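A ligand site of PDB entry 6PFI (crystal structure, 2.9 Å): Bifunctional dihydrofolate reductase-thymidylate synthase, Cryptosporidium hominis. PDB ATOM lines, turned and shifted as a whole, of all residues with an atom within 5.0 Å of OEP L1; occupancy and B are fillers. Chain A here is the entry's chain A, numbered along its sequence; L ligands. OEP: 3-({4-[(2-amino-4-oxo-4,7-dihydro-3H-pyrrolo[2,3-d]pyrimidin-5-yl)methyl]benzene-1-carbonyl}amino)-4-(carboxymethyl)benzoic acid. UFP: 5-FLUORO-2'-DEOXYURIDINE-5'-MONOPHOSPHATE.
An oxygen (O3) of OEP L1 lies close to the backbone carbonyl oxygen of Ile 515 (2.7 Å).
NZ of Lys 284 lies within salt-bridge range of O4 of OEP L1, at 2.8 Å.
O of Ala 520 lies within hydrogen-bond range of N4 of OEP L1 (3.1 Å).
OD1 of Asn 319 lies within hydrogen-bond range of N3 of OEP L1, at 3.2 Å.
An oxygen (O5) of OEP L1 sits at hydrogen-bond distance from the side-chain hydroxyl (OG) of Ser 290, at 3.2 Å.
The backbone NH (N) of Gly 430 lies within hydrogen-bond range of an oxygen (O1) of OEP L1 (3.3 Å).
OD2 of Asp 426 lies within hydrogen-bond range of N2 of OEP L1.
The backbone NH of Asp 426 lies within hydrogen-bond range of an oxygen (O2) of UFP L2, at 2.8 Å.
O3' of UFP L2 lies within hydrogen-bond range of OH of Tyr 466 (2.7 Å).
The guanidinium group (NE) of Arg 257 is in salt-bridge range of an oxygen (O1P) of UFP L2, 3.5 Å away.
An oxygen (O3') of UFP L2 is in hydrogen-bond range of a nitrogen (N4) of OEP L1, at 3.4 Å.
CB of Ala 287 touches O5 of OEP L1, 3.6 Å away.
Ile 315 touches OEP L1.
Trp 316 touches OEP L1.
Leu 399 touches OEP L1.
Leu 429 touches OEP L1 (CD2 to C20, 3.6 Å).
CZ of Phe 433 touches N5 of OEP L1, at 3.6 Å.
OH of Tyr 466 touches N4 of OEP L1, 3.6 Å away.
Met 517 touches OEP L1.
Met 519 touches OEP L1 (CG to C4, 3.8 Å).
Hydrophobic or aromatic side chains within 4 Å of OEP L1: Ala 287, Ile 315, Trp 316, Leu 399, Leu 429, Phe 433, Met 517 and Met 519.
16 residues have an atom within 4 Å of OEP L1: Lys 284, Ala 287, Ser 290, Ile 315, Trp 316, Asn 319, Leu 399, Asp 426, Leu 429, Gly 430, Phe 433, Tyr 466, Ile 515, Met 517, Met 519 and Ala 520.
The side-chain amino group (NZ) of Lys 284 lies within hydrogen-bond range of the backbone carbonyl oxygen (O) of Gly 428, 3.3 Å away.
OD1 of Asp 426 sits close to N of Gly 428 (3.2 Å).
The side-chain carboxylate (OE2) of Glu 294 lies within hydrogen-bond range of the indole nitrogen (NE1) of Trp 316 (3.2 Å).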
ATOM      1  N   ARG A 257     -32.207  10.401  -2.282  1.00  0.00           N
ATOM      2  CA  ARG A 257     -31.806  11.382  -1.273  1.00  0.00           C
ATOM      3  C   ARG A 257     -30.832  12.423  -1.809  1.00  0.00           C
ATOM      4  O   ARG A 257     -30.750  13.518  -1.250  1.00  0.00           O
ATOM      5  CB  ARG A 257     -31.200  10.664  -0.068  1.00  0.00           C
ATOM      6  CG  ARG A 257     -30.059   9.739  -0.438  1.00  0.00           C
ATOM      7  CD  ARG A 257     -29.282   9.302   0.784  1.00  0.00           C
ATOM      8  NE  ARG A 257     -28.049   8.620   0.398  1.00  0.00           N
ATOM      9  CZ  ARG A 257     -26.912   9.238   0.119  1.00  0.00           C
ATOM     10  NH1 ARG A 257     -26.843  10.561   0.181  1.00  0.00           N
ATOM     11  NH2 ARG A 257     -25.837   8.540  -0.235  1.00  0.00           N
ATOM     12  N   LYS A 284     -12.012  -0.346 -17.786  1.00  0.00           N
ATOM     13  CA  LYS A 284     -11.749   0.921 -17.135  1.00  0.00           C
ATOM     14  C   LYS A 284     -10.671   0.689 -16.085  1.00  0.00           C
ATOM     15  O   LYS A 284     -10.744  -0.286 -15.330  1.00  0.00           O
ATOM     16  CB  LYS A 284     -13.013   1.506 -16.493  1.00  0.00           C
ATOM     17  CG  LYS A 284     -12.765   2.696 -15.583  1.00  0.00           C
ATOM     18  CD  LYS A 284     -14.025   3.075 -14.821  1.00  0.00           C
ATOM     19  CE  LYS A 284     -14.531   1.929 -13.966  1.00  0.00           C
ATOM     20  NZ  LYS A 284     -15.743   2.315 -13.180  1.00  0.00           N
ATOM     21  N   ALA A 287      -8.977   1.991  -9.594  1.00  0.00           N
ATOM     22  CA  ALA A 287      -8.002   2.369  -8.573  1.00  0.00           C
ATOM     23  C   ALA A 287      -7.936   1.263  -7.530  1.00  0.00           C
ATOM     24  O   ALA A 287      -8.561   1.308  -6.469  1.00  0.00           O
ATOM     25  CB  ALA A 287      -8.379   3.705  -7.948  1.00  0.00           C
ATOM     26  N   SER A 290      -6.796   2.224  -3.783  1.00  0.00           N
ATOM     27  CA  SER A 290      -7.809   2.795  -2.896  1.00  0.00           C
ATOM     28  C   SER A 290      -8.792   1.732  -2.412  1.00  0.00           C
ATOM     29  O   SER A 290      -9.308   1.833  -1.292  1.00  0.00           O
ATOM     30  CB  SER A 290      -8.550   3.925  -3.600  1.00  0.00           C
ATOM     31  OG  SER A 290      -7.653   4.871  -4.143  1.00  0.00           O
ATOM     32  N   GLU A 294      -9.186   0.808   1.692  1.00  0.00           N
ATOM     33  CA  GLU A 294     -10.512   0.830   2.314  1.00  0.00           C
ATOM     34  C   GLU A 294     -10.839  -0.515   2.946  1.00  0.00           C
ATOM     35  O   GLU A 294     -11.432  -0.561   4.034  1.00  0.00           O
ATOM     36  CB  GLU A 294     -11.576   1.218   1.283  1.00  0.00           C
ATOM     37  CG  GLU A 294     -12.995   1.246   1.835  1.00  0.00           C
ATOM     38  CD  GLU A 294     -14.065   1.211   0.757  1.00  0.00           C
ATOM     39  OE1 GLU A 294     -13.792   0.663  -0.331  1.00  0.00           O
ATOM     40  OE2 GLU A 294     -15.175   1.719   0.998  1.00  0.00           O
ATOM     41  N   ILE A 315     -12.343   8.662  -0.964  1.00  0.00           N
ATOM     42  CA  ILE A 315     -13.661   8.159  -1.332  1.00  0.00           C
ATOM     43  C   ILE A 315     -14.708   8.424  -0.256  1.00  0.00           C
ATOM     44  O   ILE A 315     -15.903   8.476  -0.573  1.00  0.00           O
ATOM     45  CB  ILE A 315     -13.619   6.655  -1.669  1.00  0.00           C
ATOM     46  CG1 ILE A 315     -13.269   5.836  -0.420  1.00  0.00           C
ATOM     47  CG2 ILE A 315     -12.634   6.392  -2.801  1.00  0.00           C
ATOM     48  CD1 ILE A 315     -13.399   4.341  -0.629  1.00  0.00           C
ATOM     49  N   TRP A 316     -14.295   8.606   1.000  1.00  0.00           N
ATOM     50  CA  TRP A 316     -15.225   8.902   2.073  1.00  0.00           C
ATOM     51  C   TRP A 316     -15.178  10.365   2.506  1.00  0.00           C
ATOM     52  O   TRP A 316     -15.562  10.695   3.629  1.00  0.00           O
ATOM     53  CB  TRP A 316     -14.958   7.995   3.280  1.00  0.00           C
ATOM     54  CG  TRP A 316     -15.463   6.597   3.085  1.00  0.00           C
ATOM     55  CD1 TRP A 316     -14.735   5.510   2.678  1.00  0.00           C
ATOM     56  CD2 TRP A 316     -16.801   6.131   3.279  1.00  0.00           C
ATOM     57  NE1 TRP A 316     -15.542   4.400   2.616  1.00  0.00           N
ATOM     58  CE2 TRP A 316     -16.820   4.752   2.980  1.00  0.00           C
ATOM     59  CE3 TRP A 316     -17.995   6.750   3.672  1.00  0.00           C
ATOM     60  CZ2 TRP A 316     -17.974   3.982   3.060  1.00  0.00           C
ATOM     61  CZ3 TRP A 316     -19.144   5.986   3.758  1.00  0.00           C
ATOM     62  CH2 TRP A 316     -19.128   4.615   3.458  1.00  0.00           C
ATOM     63  N   ASN A 319     -19.155  11.899   2.048  1.00  0.00           N
ATOM     64  CA  ASN A 319     -20.048  11.501   3.139  1.00  0.00           C
ATOM     65  C   ASN A 319     -19.466  11.780   4.513  1.00  0.00           C
ATOM     66  O   ASN A 319     -20.028  11.326   5.511  1.00  0.00           O
ATOM     67  CB  ASN A 319     -20.386  10.006   3.012  1.00  0.00           C
ATOM     68  CG  ASN A 319     -20.923   9.649   1.642  1.00  0.00           C
ATOM     69  OD1 ASN A 319     -20.160   9.405   0.713  1.00  0.00           O
ATOM     70  ND2 ASN A 319     -22.240   9.624   1.510  1.00  0.00           N
ATOM     71  N   LEU A 399     -23.759   6.831   6.836  1.00  0.00           N
ATOM     72  CA  LEU A 399     -24.367   6.225   5.653  1.00  0.00           C
ATOM     73  C   LEU A 399     -24.637   4.756   5.954  1.00  0.00           C
ATOM     74  O   LEU A 399     -23.718   4.019   6.322  1.00  0.00           O
ATOM     75  CB  LEU A 399     -23.449   6.379   4.431  1.00  0.00           C
ATOM     76  CG  LEU A 399     -24.030   5.972   3.080  1.00  0.00           C
ATOM     77  CD1 LEU A 399     -25.233   6.842   2.738  1.00  0.00           C
ATOM     78  CD2 LEU A 399     -22.972   6.078   1.989  1.00  0.00           C
ATOM     79  N   ASP A 426     -24.326   1.563  -6.784  1.00  0.00           N
ATOM     80  CA  ASP A 426     -23.937   2.575  -7.754  1.00  0.00           C
ATOM     81  C   ASP A 426     -23.044   1.906  -8.793  1.00  0.00           C
ATOM     82  O   ASP A 426     -21.835   1.735  -8.586  1.00  0.00           O
ATOM     83  CB  ASP A 426     -23.234   3.736  -7.055  1.00  0.00           C
ATOM     84  CG  ASP A 426     -22.773   4.816  -8.019  1.00  0.00           C
ATOM     85  OD1 ASP A 426     -23.135   4.764  -9.221  1.00  0.00           O
ATOM     86  OD2 ASP A 426     -22.049   5.725  -7.569  1.00  0.00           O
ATOM     87  N   GLY A 428     -21.720   2.904 -11.403  1.00  0.00           N
ATOM     88  CA  GLY A 428     -20.656   3.700 -11.968  1.00  0.00           C
ATOM     89  C   GLY A 428     -19.400   3.721 -11.121  1.00  0.00           C
ATOM     90  O   GLY A 428     -18.289   3.672 -11.644  1.00  0.00           O
ATOM     91  N   LEU A 429     -19.565   3.776  -9.793  1.00  0.00           N
ATOM     92  CA  LEU A 429     -18.428   3.904  -8.879  1.00  0.00           C
ATOM     93  C   LEU A 429     -18.385   2.772  -7.874  1.00  0.00           C
ATOM     94  O   LEU A 429     -17.363   2.084  -7.762  1.00  0.00           O
ATOM     95  CB  LEU A 429     -18.480   5.260  -8.164  1.00  0.00           C
ATOM     96  CG  LEU A 429     -18.486   6.511  -9.029  1.00  0.00           C
ATOM     97  CD1 LEU A 429     -18.386   7.760  -8.160  1.00  0.00           C
ATOM     98  CD2 LEU A 429     -17.353   6.477 -10.040  1.00  0.00           C
ATOM     99  N   GLY A 430     -19.461   2.555  -7.107  1.00  0.00           N
ATOM    100  CA  GLY A 430     -19.397   1.578  -6.024  1.00  0.00           C
ATOM    101  C   GLY A 430     -19.244   0.152  -6.524  1.00  0.00           C
ATOM    102  O   GLY A 430     -18.526  -0.647  -5.931  1.00  0.00           O
ATOM    103  N   PRO A 432     -17.744  -1.397  -9.279  1.00  0.00           N
ATOM    104  CA  PRO A 432     -16.383  -1.903  -9.520  1.00  0.00           C
ATOM    105  C   PRO A 432     -15.538  -1.993  -8.264  1.00  0.00           C
ATOM    106  O   PRO A 432     -14.660  -2.851  -8.177  1.00  0.00           O
ATOM    107  CB  PRO A 432     -15.806  -0.908 -10.540  1.00  0.00           C
ATOM    108  CG  PRO A 432     -16.633   0.319 -10.392  1.00  0.00           C
ATOM    109  CD  PRO A 432     -18.008  -0.174 -10.062  1.00  0.00           C
ATOM    110  N   PHE A 433     -15.797  -1.134  -7.275  1.00  0.00           N
ATOM    111  CA  PHE A 433     -15.103  -1.235  -5.998  1.00  0.00           C
ATOM    112  C   PHE A 433     -15.579  -2.459  -5.210  1.00  0.00           C
ATOM    113  O   PHE A 433     -14.753  -3.176  -4.635  1.00  0.00           O
ATOM    114  CB  PHE A 433     -15.288   0.038  -5.180  1.00  0.00           C
ATOM    115  CG  PHE A 433     -14.262   1.098  -5.447  1.00  0.00           C
ATOM    116  CD1 PHE A 433     -14.026   1.541  -6.741  1.00  0.00           C
ATOM    117  CD2 PHE A 433     -13.533   1.653  -4.410  1.00  0.00           C
ATOM    118  CE1 PHE A 433     -13.075   2.513  -6.991  1.00  0.00           C
ATOM    119  CE2 PHE A 433     -12.586   2.633  -4.649  1.00  0.00           C
ATOM    120  CZ  PHE A 433     -12.353   3.062  -5.943  1.00  0.00           C
ATOM    121  N   TYR A 466     -26.471   6.590 -11.960  1.00  0.00           N
ATOM    122  CA  TYR A 466     -26.736   8.019 -11.808  1.00  0.00           C
ATOM    123  C   TYR A 466     -26.708   8.702 -13.163  1.00  0.00           C
ATOM    124  O   TYR A 466     -25.908   8.360 -14.031  1.00  0.00           O
ATOM    125  CB  TYR A 466     -25.711   8.646 -10.861  1.00  0.00           C
ATOM    126  CG  TYR A 466     -25.969   8.332  -9.413  1.00  0.00           C
ATOM    127  CD1 TYR A 466     -25.452   7.185  -8.826  1.00  0.00           C
ATOM    128  CD2 TYR A 466     -26.766   9.166  -8.636  1.00  0.00           C
ATOM    129  CE1 TYR A 466     -25.698   6.895  -7.494  1.00  0.00           C
ATOM    130  CE2 TYR A 466     -27.016   8.869  -7.310  1.00  0.00           C
ATOM    131  CZ  TYR A 466     -26.487   7.741  -6.752  1.00  0.00           C
ATOM    132  OH  TYR A 466     -26.748   7.453  -5.428  1.00  0.00           O
ATOM    133  N   THR A 514      -8.712   5.358 -17.758  1.00  0.00           N
ATOM    134  CA  THR A 514      -9.672   5.616 -16.687  1.00  0.00           C
ATOM    135  C   THR A 514     -10.783   6.532 -17.176  1.00  0.00           C
ATOM    136  O   THR A 514     -10.616   7.302 -18.120  1.00  0.00           O
ATOM    137  CB  THR A 514      -8.968   6.243 -15.481  1.00  0.00           C
ATOM    138  OG1 THR A 514      -9.940   6.594 -14.486  1.00  0.00           O
ATOM    139  CG2 THR A 514      -8.197   7.477 -15.902  1.00  0.00           C
ATOM    140  N   ILE A 515     -11.947   6.420 -16.525  1.00  0.00           N
ATOM    141  CA  ILE A 515     -13.132   7.186 -16.866  1.00  0.00           C
ATOM    142  C   ILE A 515     -13.551   7.968 -15.634  1.00  0.00           C
ATOM    143  O   ILE A 515     -13.910   7.375 -14.613  1.00  0.00           O
ATOM    144  CB  ILE A 515     -14.275   6.287 -17.357  1.00  0.00           C
ATOM    145  CG1 ILE A 515     -13.859   5.547 -18.633  1.00  0.00           C
ATOM    146  CG2 ILE A 515     -15.526   7.095 -17.598  1.00  0.00           C
ATOM    147  CD1 ILE A 515     -14.872   4.520 -19.094  1.00  0.00           C
ATOM    148  N   LYS A 516     -13.549   9.298 -15.743  1.00  0.00           N
ATOM    149  CA  LYS A 516     -13.877  10.150 -14.600  1.00  0.00           C
ATOM    150  C   LYS A 516     -15.380  10.206 -14.394  1.00  0.00           C
ATOM    151  O   LYS A 516     -16.142  10.475 -15.332  1.00  0.00           O
ATOM    152  CB  LYS A 516     -13.320  11.560 -14.813  1.00  0.00           C
ATOM    153  N   MET A 517     -15.819   9.952 -13.160  1.00  0.00           N
ATOM    154  CA  MET A 517     -17.230  10.018 -12.801  1.00  0.00           C
ATOM    155  C   MET A 517     -17.359  10.634 -11.416  1.00  0.00           C
ATOM    156  O   MET A 517     -16.635  10.249 -10.490  1.00  0.00           O
ATOM    157  CB  MET A 517     -17.893   8.642 -12.826  1.00  0.00           C
ATOM    158  CG  MET A 517     -18.025   8.032 -14.212  1.00  0.00           C
ATOM    159  SD  MET A 517     -18.769   6.392 -14.172  1.00  0.00           S
ATOM    160  CE  MET A 517     -17.388   5.375 -14.663  1.00  0.00           C
ATOM    161  N   MET A 519     -19.153  11.512  -7.798  1.00  0.00           N
ATOM    162  CA  MET A 519     -19.977  10.828  -6.807  1.00  0.00           C
ATOM    163  C   MET A 519     -21.117  11.726  -6.360  1.00  0.00           C
ATOM    164  O   MET A 519     -20.937  12.927  -6.131  1.00  0.00           O
ATOM    165  CB  MET A 519     -19.153  10.412  -5.592  1.00  0.00           C
ATOM    166  CG  MET A 519     -19.966   9.750  -4.502  1.00  0.00           C
ATOM    167  SD  MET A 519     -19.096   9.599  -2.936  1.00  0.00           S
ATOM    168  CE  MET A 519     -18.775  11.317  -2.564  1.00  0.00           C
ATOM    169  N   ALA A 520     -22.302  11.141  -6.228  1.00  0.00           N
ATOM    170  CA  ALA A 520     -23.481  11.845  -5.726  1.00  0.00           C
ATOM    171  C   ALA A 520     -23.463  11.781  -4.204  1.00  0.00           C
ATOM    172  O   ALA A 520     -23.616  10.708  -3.613  1.00  0.00           O
ATOM    173  CB  ALA A 520     -24.750  11.237  -6.293  1.00  0.00           C
HETATM  174  C1  OEP L   1     -20.940   6.421  -1.691  1.00  0.00           C
HETATM  175  C10 OEP L   1     -16.225   6.930  -3.979  1.00  0.00           C
HETATM  176  C11 OEP L   1     -15.628   6.195  -4.998  1.00  0.00           C
HETATM  177  C12 OEP L   1     -15.805   4.811  -5.049  1.00  0.00           C
HETATM  178  C13 OEP L   1     -16.558   4.167  -4.068  1.00  0.00           C
HETATM  179  C14 OEP L   1     -14.826   6.880  -6.073  1.00  0.00           C
HETATM  180  C15 OEP L   1     -13.495   6.140  -8.110  1.00  0.00           C
HETATM  181  C16 OEP L   1     -12.292   6.853  -8.163  1.00  0.00           C
HETATM  182  C17 OEP L   1     -11.612   6.932  -9.380  1.00  0.00           C
HETATM  183  C18 OEP L   1     -12.109   6.322 -10.524  1.00  0.00           C
HETATM  184  C19 OEP L   1     -13.302   5.615 -10.452  1.00  0.00           C
HETATM  185  C2  OEP L   1     -20.106   5.610  -2.469  1.00  0.00           C
HETATM  186  C20 OEP L   1     -13.977   5.528  -9.246  1.00  0.00           C
HETATM  187  C21 OEP L   1     -13.877   4.931 -11.656  1.00  0.00           C
HETATM  188  C22 OEP L   1     -11.697   7.548  -6.969  1.00  0.00           C
HETATM  189  C23 OEP L   1     -10.250   7.166  -6.802  1.00  0.00           C
HETATM  190  C3  OEP L   1     -20.443   5.441  -3.890  1.00  0.00           C
HETATM  191  C4  OEP L   1     -22.336   6.950  -3.386  1.00  0.00           C
HETATM  192  C5  OEP L   1     -19.096   5.119  -1.616  1.00  0.00           C
HETATM  193  C6  OEP L   1     -19.338   5.651  -0.354  1.00  0.00           C
HETATM  194  C7  OEP L   1     -17.957   4.217  -1.975  1.00  0.00           C
HETATM  195  C8  OEP L   1     -17.139   4.899  -3.042  1.00  0.00           C
HETATM  196  C9  OEP L   1     -16.967   6.277  -2.997  1.00  0.00           C
HETATM  197  N1  OEP L   1     -22.046   7.094  -2.134  1.00  0.00           N
HETATM  198  N2  OEP L   1     -21.559   6.161  -4.214  1.00  0.00           N
HETATM  199  N3  OEP L   1     -20.467   6.443  -0.420  1.00  0.00           N
HETATM  200  N4  OEP L   1     -23.485   7.604  -3.991  1.00  0.00           N
HETATM  201  N5  OEP L   1     -14.313   5.969  -6.908  1.00  0.00           N
HETATM  202  O1  OEP L   1     -19.849   4.782  -4.743  1.00  0.00           O
HETATM  203  O2  OEP L   1     -14.658   8.083  -6.195  1.00  0.00           O
HETATM  204  O3  OEP L   1     -14.080   5.421 -12.755  1.00  0.00           O
HETATM  205  O4  OEP L   1     -14.161   3.636 -11.353  1.00  0.00           O
HETATM  206  O5  OEP L   1      -9.773   6.374  -5.996  1.00  0.00           O
HETATM  207  O6  OEP L   1      -9.488   7.861  -7.696  1.00  0.00           O
HETATM  208  N1  UFP L   2     -22.681   2.683  -2.799  1.00  0.00           N
HETATM  209  C2  UFP L   2     -22.409   1.480  -3.363  1.00  0.00           C
HETATM  210  N3  UFP L   2     -21.474   0.673  -2.833  1.00  0.00           N
HETATM  211  C4  UFP L   2     -20.781   1.027  -1.733  1.00  0.00           C
HETATM  212  C5  UFP L   2     -21.050   2.287  -1.136  1.00  0.00           C
HETATM  213  C6  UFP L   2     -21.989   3.074  -1.689  1.00  0.00           C
HETATM  214  O2  UFP L   2     -22.982   1.065  -4.368  1.00  0.00           O
HETATM  215  O4  UFP L   2     -19.935   0.290  -1.264  1.00  0.00           O
HETATM  216  F5  UFP L   2     -20.383   2.689  -0.036  1.00  0.00           F
HETATM  217  C1' UFP L   2     -23.679   3.659  -3.287  1.00  0.00           C
HETATM  218  C2' UFP L   2     -25.090   3.088  -3.548  1.00  0.00           C
HETATM  219  C3' UFP L   2     -25.864   4.409  -3.635  1.00  0.00           C
HETATM  220  C4' UFP L   2     -25.275   5.177  -2.433  1.00  0.00           C
HETATM  221  O3' UFP L   2     -25.529   5.082  -4.837  1.00  0.00           O
HETATM  222  O4' UFP L   2     -23.936   4.633  -2.244  1.00  0.00           O
HETATM  223  C5' UFP L   2     -26.135   4.978  -1.171  1.00  0.00           C
HETATM  224  O5' UFP L   2     -27.263   5.849  -1.241  1.00  0.00           O
HETATM  225  P   UFP L   2     -28.499   5.097  -0.537  1.00  0.00           P
HETATM  226  O1P UFP L   2     -29.855   5.914  -0.827  1.00  0.00           O
HETATM  227  O2P UFP L   2     -28.629   3.731  -1.096  1.00  0.00           O
HETATM  228  O3P UFP L   2     -28.260   4.992   1.052  1.00  0.00           O
